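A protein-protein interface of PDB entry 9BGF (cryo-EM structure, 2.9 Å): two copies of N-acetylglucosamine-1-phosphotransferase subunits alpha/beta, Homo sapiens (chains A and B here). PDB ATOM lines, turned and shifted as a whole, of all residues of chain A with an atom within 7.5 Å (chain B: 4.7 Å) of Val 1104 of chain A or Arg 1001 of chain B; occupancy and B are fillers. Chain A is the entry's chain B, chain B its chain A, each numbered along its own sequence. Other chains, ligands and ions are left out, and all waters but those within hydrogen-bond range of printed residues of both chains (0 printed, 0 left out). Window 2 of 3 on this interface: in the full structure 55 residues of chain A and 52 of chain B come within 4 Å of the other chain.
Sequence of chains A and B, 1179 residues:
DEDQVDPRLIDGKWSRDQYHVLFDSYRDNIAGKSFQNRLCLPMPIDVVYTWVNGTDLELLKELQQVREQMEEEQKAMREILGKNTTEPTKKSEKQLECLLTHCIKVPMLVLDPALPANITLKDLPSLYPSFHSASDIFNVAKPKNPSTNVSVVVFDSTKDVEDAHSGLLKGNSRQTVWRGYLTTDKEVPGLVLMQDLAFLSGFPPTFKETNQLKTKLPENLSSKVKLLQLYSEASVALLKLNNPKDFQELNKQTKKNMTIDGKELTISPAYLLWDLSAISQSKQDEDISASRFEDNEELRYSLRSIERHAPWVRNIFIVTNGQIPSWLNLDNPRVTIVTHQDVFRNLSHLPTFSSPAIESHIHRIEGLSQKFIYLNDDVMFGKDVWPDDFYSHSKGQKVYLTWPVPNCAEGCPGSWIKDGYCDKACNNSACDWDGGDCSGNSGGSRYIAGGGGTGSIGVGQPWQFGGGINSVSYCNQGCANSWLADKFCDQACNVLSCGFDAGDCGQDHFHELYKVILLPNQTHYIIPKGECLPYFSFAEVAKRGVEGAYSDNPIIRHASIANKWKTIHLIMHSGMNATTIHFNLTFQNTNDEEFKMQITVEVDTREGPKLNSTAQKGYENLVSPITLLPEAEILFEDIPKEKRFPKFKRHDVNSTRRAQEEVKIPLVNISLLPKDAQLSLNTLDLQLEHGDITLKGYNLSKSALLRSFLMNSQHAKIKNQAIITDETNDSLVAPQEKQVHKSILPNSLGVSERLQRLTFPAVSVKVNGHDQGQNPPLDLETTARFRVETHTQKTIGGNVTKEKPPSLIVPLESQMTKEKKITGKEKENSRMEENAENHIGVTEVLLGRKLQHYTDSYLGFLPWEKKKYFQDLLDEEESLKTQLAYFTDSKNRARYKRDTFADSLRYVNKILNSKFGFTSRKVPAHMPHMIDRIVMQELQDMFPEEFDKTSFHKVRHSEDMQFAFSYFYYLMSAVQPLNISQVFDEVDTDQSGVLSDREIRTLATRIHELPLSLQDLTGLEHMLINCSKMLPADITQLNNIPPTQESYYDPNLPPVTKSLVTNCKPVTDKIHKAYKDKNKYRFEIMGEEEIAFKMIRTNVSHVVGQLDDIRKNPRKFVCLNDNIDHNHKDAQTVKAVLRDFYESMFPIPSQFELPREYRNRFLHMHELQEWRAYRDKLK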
ATOM      1  N   ASN A1099      30.462   9.303   1.180  1.00  0.00           N
ATOM      2  CA  ASN A1099      29.079   9.772   1.221  1.00  0.00           C
ATOM      3  C   ASN A1099      28.335   8.881   2.204  1.00  0.00           C
ATOM      4  O   ASN A1099      28.130   7.697   1.929  1.00  0.00           O
ATOM      5  CB  ASN A1099      28.442   9.734  -0.169  1.00  0.00           C
ATOM      6  CG  ASN A1099      27.005  10.231  -0.182  1.00  0.00           C
ATOM      7  OD1 ASN A1099      26.197   9.880   0.677  1.00  0.00           O
ATOM      8  ND2 ASN A1099      26.678  11.045  -1.175  1.00  0.00           N
ATOM      9  N   VAL A1100      27.911   9.450   3.333  1.00  0.00           N
ATOM     10  CA  VAL A1100      27.372   8.639   4.424  1.00  0.00           C
ATOM     11  C   VAL A1100      26.127   7.881   3.974  1.00  0.00           C
ATOM     12  O   VAL A1100      25.995   6.676   4.217  1.00  0.00           O
ATOM     13  CB  VAL A1100      27.089   9.517   5.655  1.00  0.00           C
ATOM     14  CG1 VAL A1100      26.420   8.696   6.741  1.00  0.00           C
ATOM     15  CG2 VAL A1100      28.380  10.126   6.168  1.00  0.00           C
ATOM     16  N   SER A1101      25.196   8.571   3.311  1.00  0.00           N
ATOM     17  CA  SER A1101      23.963   7.911   2.894  1.00  0.00           C
ATOM     18  C   SER A1101      24.239   6.818   1.868  1.00  0.00           C
ATOM     19  O   SER A1101      23.694   5.712   1.965  1.00  0.00           O
ATOM     20  CB  SER A1101      22.975   8.937   2.337  1.00  0.00           C
ATOM     21  OG  SER A1101      23.475   9.542   1.158  1.00  0.00           O
ATOM     22  N   HIS A1102      25.091   7.105   0.881  1.00  0.00           N
ATOM     23  CA  HIS A1102      25.410   6.110  -0.137  1.00  0.00           C
ATOM     24  C   HIS A1102      26.182   4.936   0.457  1.00  0.00           C
ATOM     25  O   HIS A1102      25.951   3.778   0.080  1.00  0.00           O
ATOM     26  CB  HIS A1102      26.202   6.767  -1.266  1.00  0.00           C
ATOM     27  CG  HIS A1102      26.175   6.001  -2.550  1.00  0.00           C
ATOM     28  ND1 HIS A1102      27.223   5.208  -2.966  1.00  0.00           N
ATOM     29  CD2 HIS A1102      25.228   5.908  -3.513  1.00  0.00           C
ATOM     30  CE1 HIS A1102      26.922   4.659  -4.129  1.00  0.00           C
ATOM     31  NE2 HIS A1102      25.717   5.068  -4.483  1.00  0.00           N
ATOM     32  N   VAL A1103      27.103   5.213   1.382  1.00  0.00           N
ATOM     33  CA  VAL A1103      27.839   4.139   2.042  1.00  0.00           C
ATOM     34  C   VAL A1103      26.887   3.245   2.822  1.00  0.00           C
ATOM     35  O   VAL A1103      26.977   2.013   2.757  1.00  0.00           O
ATOM     36  CB  VAL A1103      28.941   4.720   2.947  1.00  0.00           C
ATOM     37  CG1 VAL A1103      29.504   3.647   3.855  1.00  0.00           C
ATOM     38  CG2 VAL A1103      30.042   5.325   2.106  1.00  0.00           C
ATOM     39  N   VAL A1104      25.960   3.850   3.566  1.00  0.00           N
ATOM     40  CA  VAL A1104      24.966   3.070   4.300  1.00  0.00           C
ATOM     41  C   VAL A1104      24.132   2.235   3.339  1.00  0.00           C
ATOM     42  O   VAL A1104      23.845   1.063   3.603  1.00  0.00           O
ATOM     43  CB  VAL A1104      24.088   3.999   5.158  1.00  0.00           C
ATOM     44  CG1 VAL A1104      22.851   3.268   5.642  1.00  0.00           C
ATOM     45  CG2 VAL A1104      24.877   4.525   6.339  1.00  0.00           C
ATOM     46  N   GLY A1105      23.746   2.818   2.203  1.00  0.00           N
ATOM     47  CA  GLY A1105      22.940   2.082   1.243  1.00  0.00           C
ATOM     48  C   GLY A1105      23.651   0.865   0.682  1.00  0.00           C
ATOM     49  O   GLY A1105      23.075  -0.221   0.588  1.00  0.00           O
ATOM     50  N   GLN A1106      24.921   1.024   0.306  1.00  0.00           N
ATOM     51  CA  GLN A1106      25.638  -0.104  -0.286  1.00  0.00           C
ATOM     52  C   GLN A1106      25.995  -1.155   0.765  1.00  0.00           C
ATOM     53  O   GLN A1106      25.997  -2.360   0.475  1.00  0.00           O
ATOM     54  CB  GLN A1106      26.877   0.386  -1.032  1.00  0.00           C
ATOM     55  CG  GLN A1106      27.852   1.193  -0.215  1.00  0.00           C
ATOM     56  CD  GLN A1106      28.883   1.884  -1.081  1.00  0.00           C
ATOM     57  OE1 GLN A1106      28.641   2.151  -2.255  1.00  0.00           O
ATOM     58  NE2 GLN A1106      30.043   2.170  -0.507  1.00  0.00           N
ATOM     59  N   LEU A1107      26.288  -0.730   1.994  1.00  0.00           N
ATOM     60  CA  LEU A1107      26.474  -1.703   3.065  1.00  0.00           C
ATOM     61  C   LEU A1107      25.184  -2.468   3.336  1.00  0.00           C
ATOM     62  O   LEU A1107      25.214  -3.668   3.628  1.00  0.00           O
ATOM     63  CB  LEU A1107      26.975  -1.009   4.328  1.00  0.00           C
ATOM     64  CG  LEU A1107      28.377  -0.410   4.215  1.00  0.00           C
ATOM     65  CD1 LEU A1107      28.821   0.168   5.541  1.00  0.00           C
ATOM     66  CD2 LEU A1107      29.367  -1.450   3.723  1.00  0.00           C
ATOM     67  N   ASP A1108      24.037  -1.790   3.241  1.00  0.00           N
ATOM     68  CA  ASP A1108      22.755  -2.478   3.352  1.00  0.00           C
ATOM     69  C   ASP A1108      22.548  -3.446   2.199  1.00  0.00           C
ATOM     70  O   ASP A1108      21.917  -4.494   2.366  1.00  0.00           O
ATOM     71  CB  ASP A1108      21.616  -1.462   3.408  1.00  0.00           C
ATOM     72  CG  ASP A1108      21.578  -0.709   4.714  1.00  0.00           C
ATOM     73  OD1 ASP A1108      22.374  -1.045   5.614  1.00  0.00           O
ATOM     74  OD2 ASP A1108      20.754   0.219   4.843  1.00  0.00           O
ATOM     75  N   ASP A1109      23.038  -3.092   1.012  1.00  0.00           N
ATOM     76  CA  ASP A1109      22.969  -4.020  -0.113  1.00  0.00           C
ATOM     77  C   ASP A1109      23.777  -5.278   0.170  1.00  0.00           C
ATOM     78  O   ASP A1109      23.367  -6.385  -0.196  1.00  0.00           O
ATOM     79  CB  ASP A1109      23.460  -3.345  -1.390  1.00  0.00           C
ATOM     80  CG  ASP A1109      22.937  -4.023  -2.637  1.00  0.00           C
ATOM     81  OD1 ASP A1109      21.995  -3.484  -3.254  1.00  0.00           O
ATOM     82  OD2 ASP A1109      23.453  -5.104  -2.988  1.00  0.00           O
ATOM     83  N   ILE A1110      24.937  -5.124   0.805  1.00  0.00           N
ATOM     84  CA  ILE A1110      25.700  -6.297   1.233  1.00  0.00           C
ATOM     85  C   ILE A1110      24.929  -7.084   2.288  1.00  0.00           C
ATOM     86  O   ILE A1110      24.909  -8.320   2.270  1.00  0.00           O
ATOM     87  CB  ILE A1110      27.093  -5.890   1.739  1.00  0.00           C
ATOM     88  CG1 ILE A1110      27.885  -5.219   0.621  1.00  0.00           C
ATOM     89  CG2 ILE A1110      27.848  -7.105   2.248  1.00  0.00           C
ATOM     90  CD1 ILE A1110      29.316  -4.948   0.971  1.00  0.00           C
ATOM     91  N   ARG A1111      24.297  -6.383   3.233  1.00  0.00           N
ATOM     92  CA  ARG A1111      23.550  -7.056   4.296  1.00  0.00           C
ATOM     93  C   ARG A1111      22.398  -7.885   3.740  1.00  0.00           C
ATOM     94  O   ARG A1111      22.195  -9.033   4.149  1.00  0.00           O
ATOM     95  CB  ARG A1111      23.014  -6.029   5.293  1.00  0.00           C
ATOM     96  CG  ARG A1111      24.070  -5.271   6.070  1.00  0.00           C
ATOM     97  CD  ARG A1111      23.451  -4.086   6.793  1.00  0.00           C
ATOM     98  NE  ARG A1111      23.532  -4.229   8.241  1.00  0.00           N
ATOM     99  CZ  ARG A1111      24.231  -3.430   9.033  1.00  0.00           C
ATOM    100  NH1 ARG A1111      24.887  -2.386   8.557  1.00  0.00           N
ATOM    101  NH2 ARG A1111      24.265  -3.680  10.337  1.00  0.00           N
ATOM    102  N   LYS A1112      21.622  -7.312   2.817  1.00  0.00           N
ATOM    103  CA  LYS A1112      20.456  -8.007   2.281  1.00  0.00           C
ATOM    104  C   LYS A1112      20.858  -9.223   1.458  1.00  0.00           C
ATOM    105  O   LYS A1112      20.231 -10.284   1.560  1.00  0.00           O
ATOM    106  CB  LYS A1112      19.617  -7.047   1.441  1.00  0.00           C
ATOM    107  CG  LYS A1112      18.382  -7.681   0.834  1.00  0.00           C
ATOM    108  CD  LYS A1112      17.588  -6.672   0.031  1.00  0.00           C
ATOM    109  CE  LYS A1112      16.301  -7.280  -0.488  1.00  0.00           C
ATOM    110  NZ  LYS A1112      15.457  -7.806   0.618  1.00  0.00           N
ATOM    111  N   THR A1133      32.623   9.726  10.307  1.00  0.00           N
ATOM    112  CA  THR A1133      31.294   9.123  10.260  1.00  0.00           C
ATOM    113  C   THR A1133      31.280   7.901   9.351  1.00  0.00           C
ATOM    114  O   THR A1133      30.649   6.888   9.670  1.00  0.00           O
ATOM    115  CB  THR A1133      30.257  10.144   9.795  1.00  0.00           C
ATOM    116  OG1 THR A1133      30.606  10.623   8.490  1.00  0.00           O
ATOM    117  CG2 THR A1133      30.187  11.315  10.762  1.00  0.00           C
ATOM    118  N   VAL A1134      31.975   7.979   8.215  1.00  0.00           N
ATOM    119  CA  VAL A1134      32.064   6.834   7.312  1.00  0.00           C
ATOM    120  C   VAL A1134      32.797   5.680   7.984  1.00  0.00           C
ATOM    121  O   VAL A1134      32.404   4.516   7.853  1.00  0.00           O
ATOM    122  CB  VAL A1134      32.738   7.248   5.994  1.00  0.00           C
ATOM    123  CG1 VAL A1134      33.101   6.029   5.186  1.00  0.00           C
ATOM    124  CG2 VAL A1134      31.820   8.151   5.196  1.00  0.00           C
ATOM    125  N   VAL A1137      30.421   4.091  10.396  1.00  0.00           N
ATOM    126  CA  VAL A1137      29.454   3.267   9.675  1.00  0.00           C
ATOM    127  C   VAL A1137      30.079   1.936   9.276  1.00  0.00           C
ATOM    128  O   VAL A1137      29.472   0.869   9.445  1.00  0.00           O
ATOM    129  CB  VAL A1137      28.917   4.030   8.449  1.00  0.00           C
ATOM    130  CG1 VAL A1137      28.128   3.105   7.554  1.00  0.00           C
ATOM    131  CG2 VAL A1137      28.056   5.193   8.888  1.00  0.00           C
ATOM    132  N   LEU A1138      31.302   1.975   8.744  1.00  0.00           N
ATOM    133  CA  LEU A1138      31.988   0.745   8.361  1.00  0.00           C
ATOM    134  C   LEU A1138      32.243  -0.146   9.569  1.00  0.00           C
ATOM    135  O   LEU A1138      32.091  -1.368   9.488  1.00  0.00           O
ATOM    136  CB  LEU A1138      33.304   1.069   7.653  1.00  0.00           C
ATOM    137  CG  LEU A1138      33.223   1.605   6.226  1.00  0.00           C
ATOM    138  CD1 LEU A1138      34.595   2.053   5.760  1.00  0.00           C
ATOM    139  CD2 LEU A1138      32.663   0.547   5.297  1.00  0.00           C
ATOM    140  N   ASP A1140      30.509  -0.247  12.361  1.00  0.00           N
ATOM    141  CA  ASP A1140      29.234  -0.813  12.790  1.00  0.00           C
ATOM    142  C   ASP A1140      28.811  -1.962  11.884  1.00  0.00           C
ATOM    143  O   ASP A1140      28.330  -2.995  12.361  1.00  0.00           O
ATOM    144  CB  ASP A1140      28.162   0.276  12.817  1.00  0.00           C
ATOM    145  CG  ASP A1140      27.106   0.025  13.871  1.00  0.00           C
ATOM    146  OD1 ASP A1140      27.367  -0.764  14.801  1.00  0.00           O
ATOM    147  OD2 ASP A1140      26.012   0.614  13.766  1.00  0.00           O
ATOM    148  N   PHE A1141      28.988  -1.800  10.572  1.00  0.00           N
ATOM    149  CA  PHE A1141      28.684  -2.871   9.626  1.00  0.00           C
ATOM    150  C   PHE A1141      29.547  -4.104   9.888  1.00  0.00           C
ATOM    151  O   PHE A1141      29.048  -5.240   9.926  1.00  0.00           O
ATOM    152  CB  PHE A1141      28.881  -2.338   8.207  1.00  0.00           C
ATOM    153  CG  PHE A1141      28.874  -3.387   7.142  1.00  0.00           C
ATOM    154  CD1 PHE A1141      27.683  -3.865   6.628  1.00  0.00           C
ATOM    155  CD2 PHE A1141      30.063  -3.864   6.617  1.00  0.00           C
ATOM    156  CE1 PHE A1141      27.679  -4.818   5.633  1.00  0.00           C
ATOM    157  CE2 PHE A1141      30.063  -4.816   5.622  1.00  0.00           C
ATOM    158  CZ  PHE A1141      28.869  -5.289   5.127  1.00  0.00           C
ATOM    159  N   SER A1144      28.418  -5.807  13.028  1.00  0.00           N
ATOM    160  CA  SER A1144      27.194  -6.555  12.773  1.00  0.00           C
ATOM    161  C   SER A1144      27.501  -7.893  12.119  1.00  0.00           C
ATOM    162  O   SER A1144      26.923  -8.919  12.493  1.00  0.00           O
ATOM    163  CB  SER A1144      26.250  -5.740  11.894  1.00  0.00           C
ATOM    164  OG  SER A1144      26.713  -5.693  10.558  1.00  0.00           O
ATOM    165  N   ASP B 997      20.940  -3.238  17.708  1.00  0.00           N
ATOM    166  CA  ASP B 997      20.490  -2.273  16.710  1.00  0.00           C
ATOM    167  C   ASP B 997      21.052  -2.601  15.332  1.00  0.00           C
ATOM    168  O   ASP B 997      20.340  -2.510  14.325  1.00  0.00           O
ATOM    169  CB  ASP B 997      20.892  -0.861  17.127  1.00  0.00           C
ATOM    170  CG  ASP B 997      20.419  -0.513  18.520  1.00  0.00           C
ATOM    171  OD1 ASP B 997      20.966  -1.072  19.494  1.00  0.00           O
ATOM    172  OD2 ASP B 997      19.500   0.322  18.638  1.00  0.00           O
ATOM    173  N   ARG B 998      22.330  -2.981  15.271  1.00  0.00           N
ATOM    174  CA  ARG B 998      22.931  -3.382  14.002  1.00  0.00           C
ATOM    175  C   ARG B 998      22.264  -4.637  13.448  1.00  0.00           C
ATOM    176  O   ARG B 998      21.993  -4.728  12.244  1.00  0.00           O
ATOM    177  CB  ARG B 998      24.431  -3.600  14.194  1.00  0.00           C
ATOM    178  CG  ARG B 998      24.759  -4.533  15.347  1.00  0.00           C
ATOM    179  CD  ARG B 998      26.222  -4.496  15.722  1.00  0.00           C
ATOM    180  NE  ARG B 998      26.643  -3.163  16.133  1.00  0.00           N
ATOM    181  CZ  ARG B 998      27.656  -2.922  16.952  1.00  0.00           C
ATOM    182  NH1 ARG B 998      28.354  -3.905  17.497  1.00  0.00           N
ATOM    183  NH2 ARG B 998      27.975  -1.662  17.236  1.00  0.00           N
ATOM    184  N   GLU B 999      21.977  -5.608  14.315  1.00  0.00           N
ATOM    185  CA  GLU B 999      21.316  -6.829  13.869  1.00  0.00           C
ATOM    186  C   GLU B 999      19.873  -6.557  13.459  1.00  0.00           C
ATOM    187  O   GLU B 999      19.366  -7.167  12.511  1.00  0.00           O
ATOM    188  CB  GLU B 999      21.397  -7.881  14.971  1.00  0.00           C
ATOM    189  CG  GLU B 999      22.825  -8.157  15.403  1.00  0.00           C
ATOM    190  CD  GLU B 999      22.923  -9.100  16.577  1.00  0.00           C
ATOM    191  OE1 GLU B 999      21.878  -9.450  17.154  1.00  0.00           O
ATOM    192  OE2 GLU B 999      24.055  -9.493  16.926  1.00  0.00           O
ATOM    193  N   ILE B1000      19.200  -5.637  14.154  1.00  0.00           N
ATOM    194  CA  ILE B1000      17.857  -5.238  13.741  1.00  0.00           C
ATOM    195  C   ILE B1000      17.899  -4.569  12.373  1.00  0.00           C
ATOM    196  O   ILE B1000      17.003  -4.761  11.547  1.00  0.00           O
ATOM    197  CB  ILE B1000      17.213  -4.329  14.804  1.00  0.00           C
ATOM    198  CG1 ILE B1000      16.910  -5.127  16.071  1.00  0.00           C
ATOM    199  CG2 ILE B1000      15.935  -3.698  14.275  1.00  0.00           C
ATOM    200  CD1 ILE B1000      16.319  -4.295  17.175  1.00  0.00           C
ATOM    201  N   ARG B1001      18.935  -3.769  12.113  1.00  0.00           N
ATOM    202  CA  ARG B1001      19.069  -3.160  10.793  1.00  0.00           C
ATOM    203  C   ARG B1001      19.328  -4.215   9.725  1.00  0.00           C
ATOM    204  O   ARG B1001      18.805  -4.118   8.608  1.00  0.00           O
ATOM    205  CB  ARG B1001      20.181  -2.111  10.802  1.00  0.00           C
ATOM    206  CG  ARG B1001      20.617  -1.662   9.416  1.00  0.00           C
ATOM    207  CD  ARG B1001      21.442  -0.390   9.467  1.00  0.00           C
ATOM    208  NE  ARG B1001      20.602   0.798   9.391  1.00  0.00           N
ATOM    209  CZ  ARG B1001      20.247   1.389   8.258  1.00  0.00           C
ATOM    210  NH1 ARG B1001      20.644   0.930   7.086  1.00  0.00           N
ATOM    211  NH2 ARG B1001      19.473   2.469   8.306  1.00  0.00           N
ATOM    212  N   THR B1002      20.125  -5.233  10.051  1.00  0.00           N
ATOM    213  CA  THR B1002      20.326  -6.335   9.115  1.00  0.00           C
ATOM    214  C   THR B1002      19.008  -7.036   8.808  1.00  0.00           C
ATOM    215  O   THR B1002      18.704  -7.324   7.644  1.00  0.00           O
ATOM    216  CB  THR B1002      21.337  -7.335   9.674  1.00  0.00           C
ATOM    217  OG1 THR B1002      22.517  -6.642  10.093  1.00  0.00           O
ATOM    218  CG2 THR B1002      21.709  -8.355   8.615  1.00  0.00           C
ATOM    219  N   LEU B1003      18.205  -7.302   9.843  1.00  0.00           N
ATOM    220  CA  LEU B1003      16.910  -7.944   9.636  1.00  0.00           C
ATOM    221  C   LEU B1003      15.982  -7.068   8.802  1.00  0.00           C
ATOM    222  O   LEU B1003      15.257  -7.567   7.934  1.00  0.00           O
ATOM    223  CB  LEU B1003      16.267  -8.272  10.982  1.00  0.00           C
ATOM    224  CG  LEU B1003      14.869  -8.890  10.930  1.00  0.00           C
ATOM    225  CD1 LEU B1003      14.891 -10.212  10.182  1.00  0.00           C
ATOM    226  CD2 LEU B1003      14.314  -9.070  12.332  1.00  0.00           C
ATOM    227  N   ALA B1004      15.985  -5.758   9.055  1.00  0.00           N
ATOM    228  CA  ALA B1004      15.159  -4.846   8.272  1.00  0.00           C
ATOM    229  C   ALA B1004      15.579  -4.839   6.809  1.00  0.00           C
ATOM    230  O   ALA B1004      14.730  -4.776   5.914  1.00  0.00           O
ATOM    231  CB  ALA B1004      15.232  -3.437   8.857  1.00  0.00           C
ATOM    232  N   THR B1005      16.888  -4.879   6.548  1.00  0.00           N
ATOM    233  CA  THR B1005      17.358  -4.967   5.168  1.00  0.00           C
ATOM    234  C   THR B1005      16.919  -6.273   4.521  1.00  0.00           C
ATOM    235  O   THR B1005      16.526  -6.292   3.349  1.00  0.00           O
ATOM    236  CB  THR B1005      18.878  -4.831   5.112  1.00  0.00           C
ATOM    237  OG1 THR B1005      19.474  -5.759   6.024  1.00  0.00           O
ATOM    238  CG2 THR B1005      19.299  -3.421   5.479  1.00  0.00           C
ATOM    239  N   LEU B1012      16.624   0.999   2.302  1.00  0.00           N
ATOM    240  CA  LEU B1012      15.958   0.916   3.599  1.00  0.00           C
ATOM    241  C   LEU B1012      15.815   2.325   4.161  1.00  0.00           C
ATOM    242  O   LEU B1012      16.744   2.867   4.763  1.00  0.00           O
ATOM    243  CB  LEU B1012      16.740   0.019   4.552  1.00  0.00           C
ATOM    244  CG  LEU B1012      16.173  -0.107   5.968  1.00  0.00           C
ATOM    245  CD1 LEU B1012      14.831  -0.817   5.946  1.00  0.00           C
ATOM    246  CD2 LEU B1012      17.142  -0.818   6.896  1.00  0.00           C
ATOM    247  N   LEU B1017      12.417   1.113   8.883  1.00  0.00           N
ATOM    248  CA  LEU B1017      13.000   0.642  10.135  1.00  0.00           C
ATOM    249  C   LEU B1017      12.174   1.094  11.332  1.00  0.00           C
ATOM    250  O   LEU B1017      11.977   0.332  12.287  1.00  0.00           O
ATOM    251  CB  LEU B1017      14.442   1.131  10.259  1.00  0.00           C
ATOM    252  CG  LEU B1017      15.200   0.653  11.495  1.00  0.00           C
ATOM    253  CD1 LEU B1017      15.212  -0.862  11.555  1.00  0.00           C
ATOM    254  CD2 LEU B1017      16.616   1.200  11.498  1.00  0.00           C
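The guanidinium group of Arg 1111 of chain A sits at hydrogen-bond distance from the backbone carbonyl oxygen of Arg 998 of chain B (3.1 Å).
NH2 of Arg 998 of chain B lies within salt-bridge range of OD1 of Asp 1140 of chain A.
The side-chain carboxylate (OD1) of Asp 1108 of chain A lies within salt-bridge range of the guanidinium group (NH1) of Arg 1001 of chain B (3.0 Å).
The guanidinium group (NE) of Arg 1111 of chain A lies within hydrogen-bond range of the side-chain hydroxyl (OG1) of Thr 1002 of chain B (3.2 Å).
The backbone carbonyl oxygen of Thr 1005 of chain B lies within hydrogen-bond range of the side-chain amino group of Lys 1112 of chain A.
The backbone carbonyl oxygen (O) of Arg 998 of chain B lies within hydrogen-bond range of the side-chain hydroxyl (OG1) of Thr 1002 of chain B.
O of Arg 1001 of chain B sits at hydrogen-bond distance from OG1 of Thr 1005 of chain B.
The side-chain hydroxyl of Ser 1144 of chain A is in hydrogen-bond range of the guanidinium group of Arg 1111 of chain A (3.2 Å).
The backbone carbonyl oxygen (O) of Phe 1141 of chain A lies within hydrogen-bond range of the side-chain hydroxyl (OG) of Ser 1144 of chain A (2.5 Å).
Among the printed residues, pairs that only touch across the chains: Val 1104 of chain A with Arg 1001 of chain B (3.5 Å), Asp 1108 of chain A with Thr 1005 of chain B (3.6 Å), Arg 1111 of chain A with Thr 1005 of chain B (3.6 Å) and Ser 1144 of chain A with Arg 998 of chain B (3.6 Å).
Val 1104 of chain A touches just one residue of chain B: Arg 1001.
Printed residues of chain B within 4 Å of Arg 1111 of chain A: Arg 998 (3.1 Å), Thr 1002 (3.2 Å) and Thr 1005 (3.6 Å).
Of the printed residues of chain B, Asp 1108 of chain A touches Arg 1001 and Thr 1005.
The nearest printed residue of chain B that does not touch Val 1104 of chain A is Leu 1012 of chain B (6.2 Å).
Hydrophobic or aromatic side chains of chain A within 4 Å of the printed part of chain B: Val 1104.
Of the 11 printed residues of chain B, 4 touch a printed residue of chain A.
Among the printed residues, Asp or Glu carboxylates within 4 Å of a Lys or Arg side-chain nitrogen of the other chain: Asp 1108 of chain A with Arg 1001 of chain B and Asp 1140 of chain A with Arg 998 of chain B.
No position is printed for both chains.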
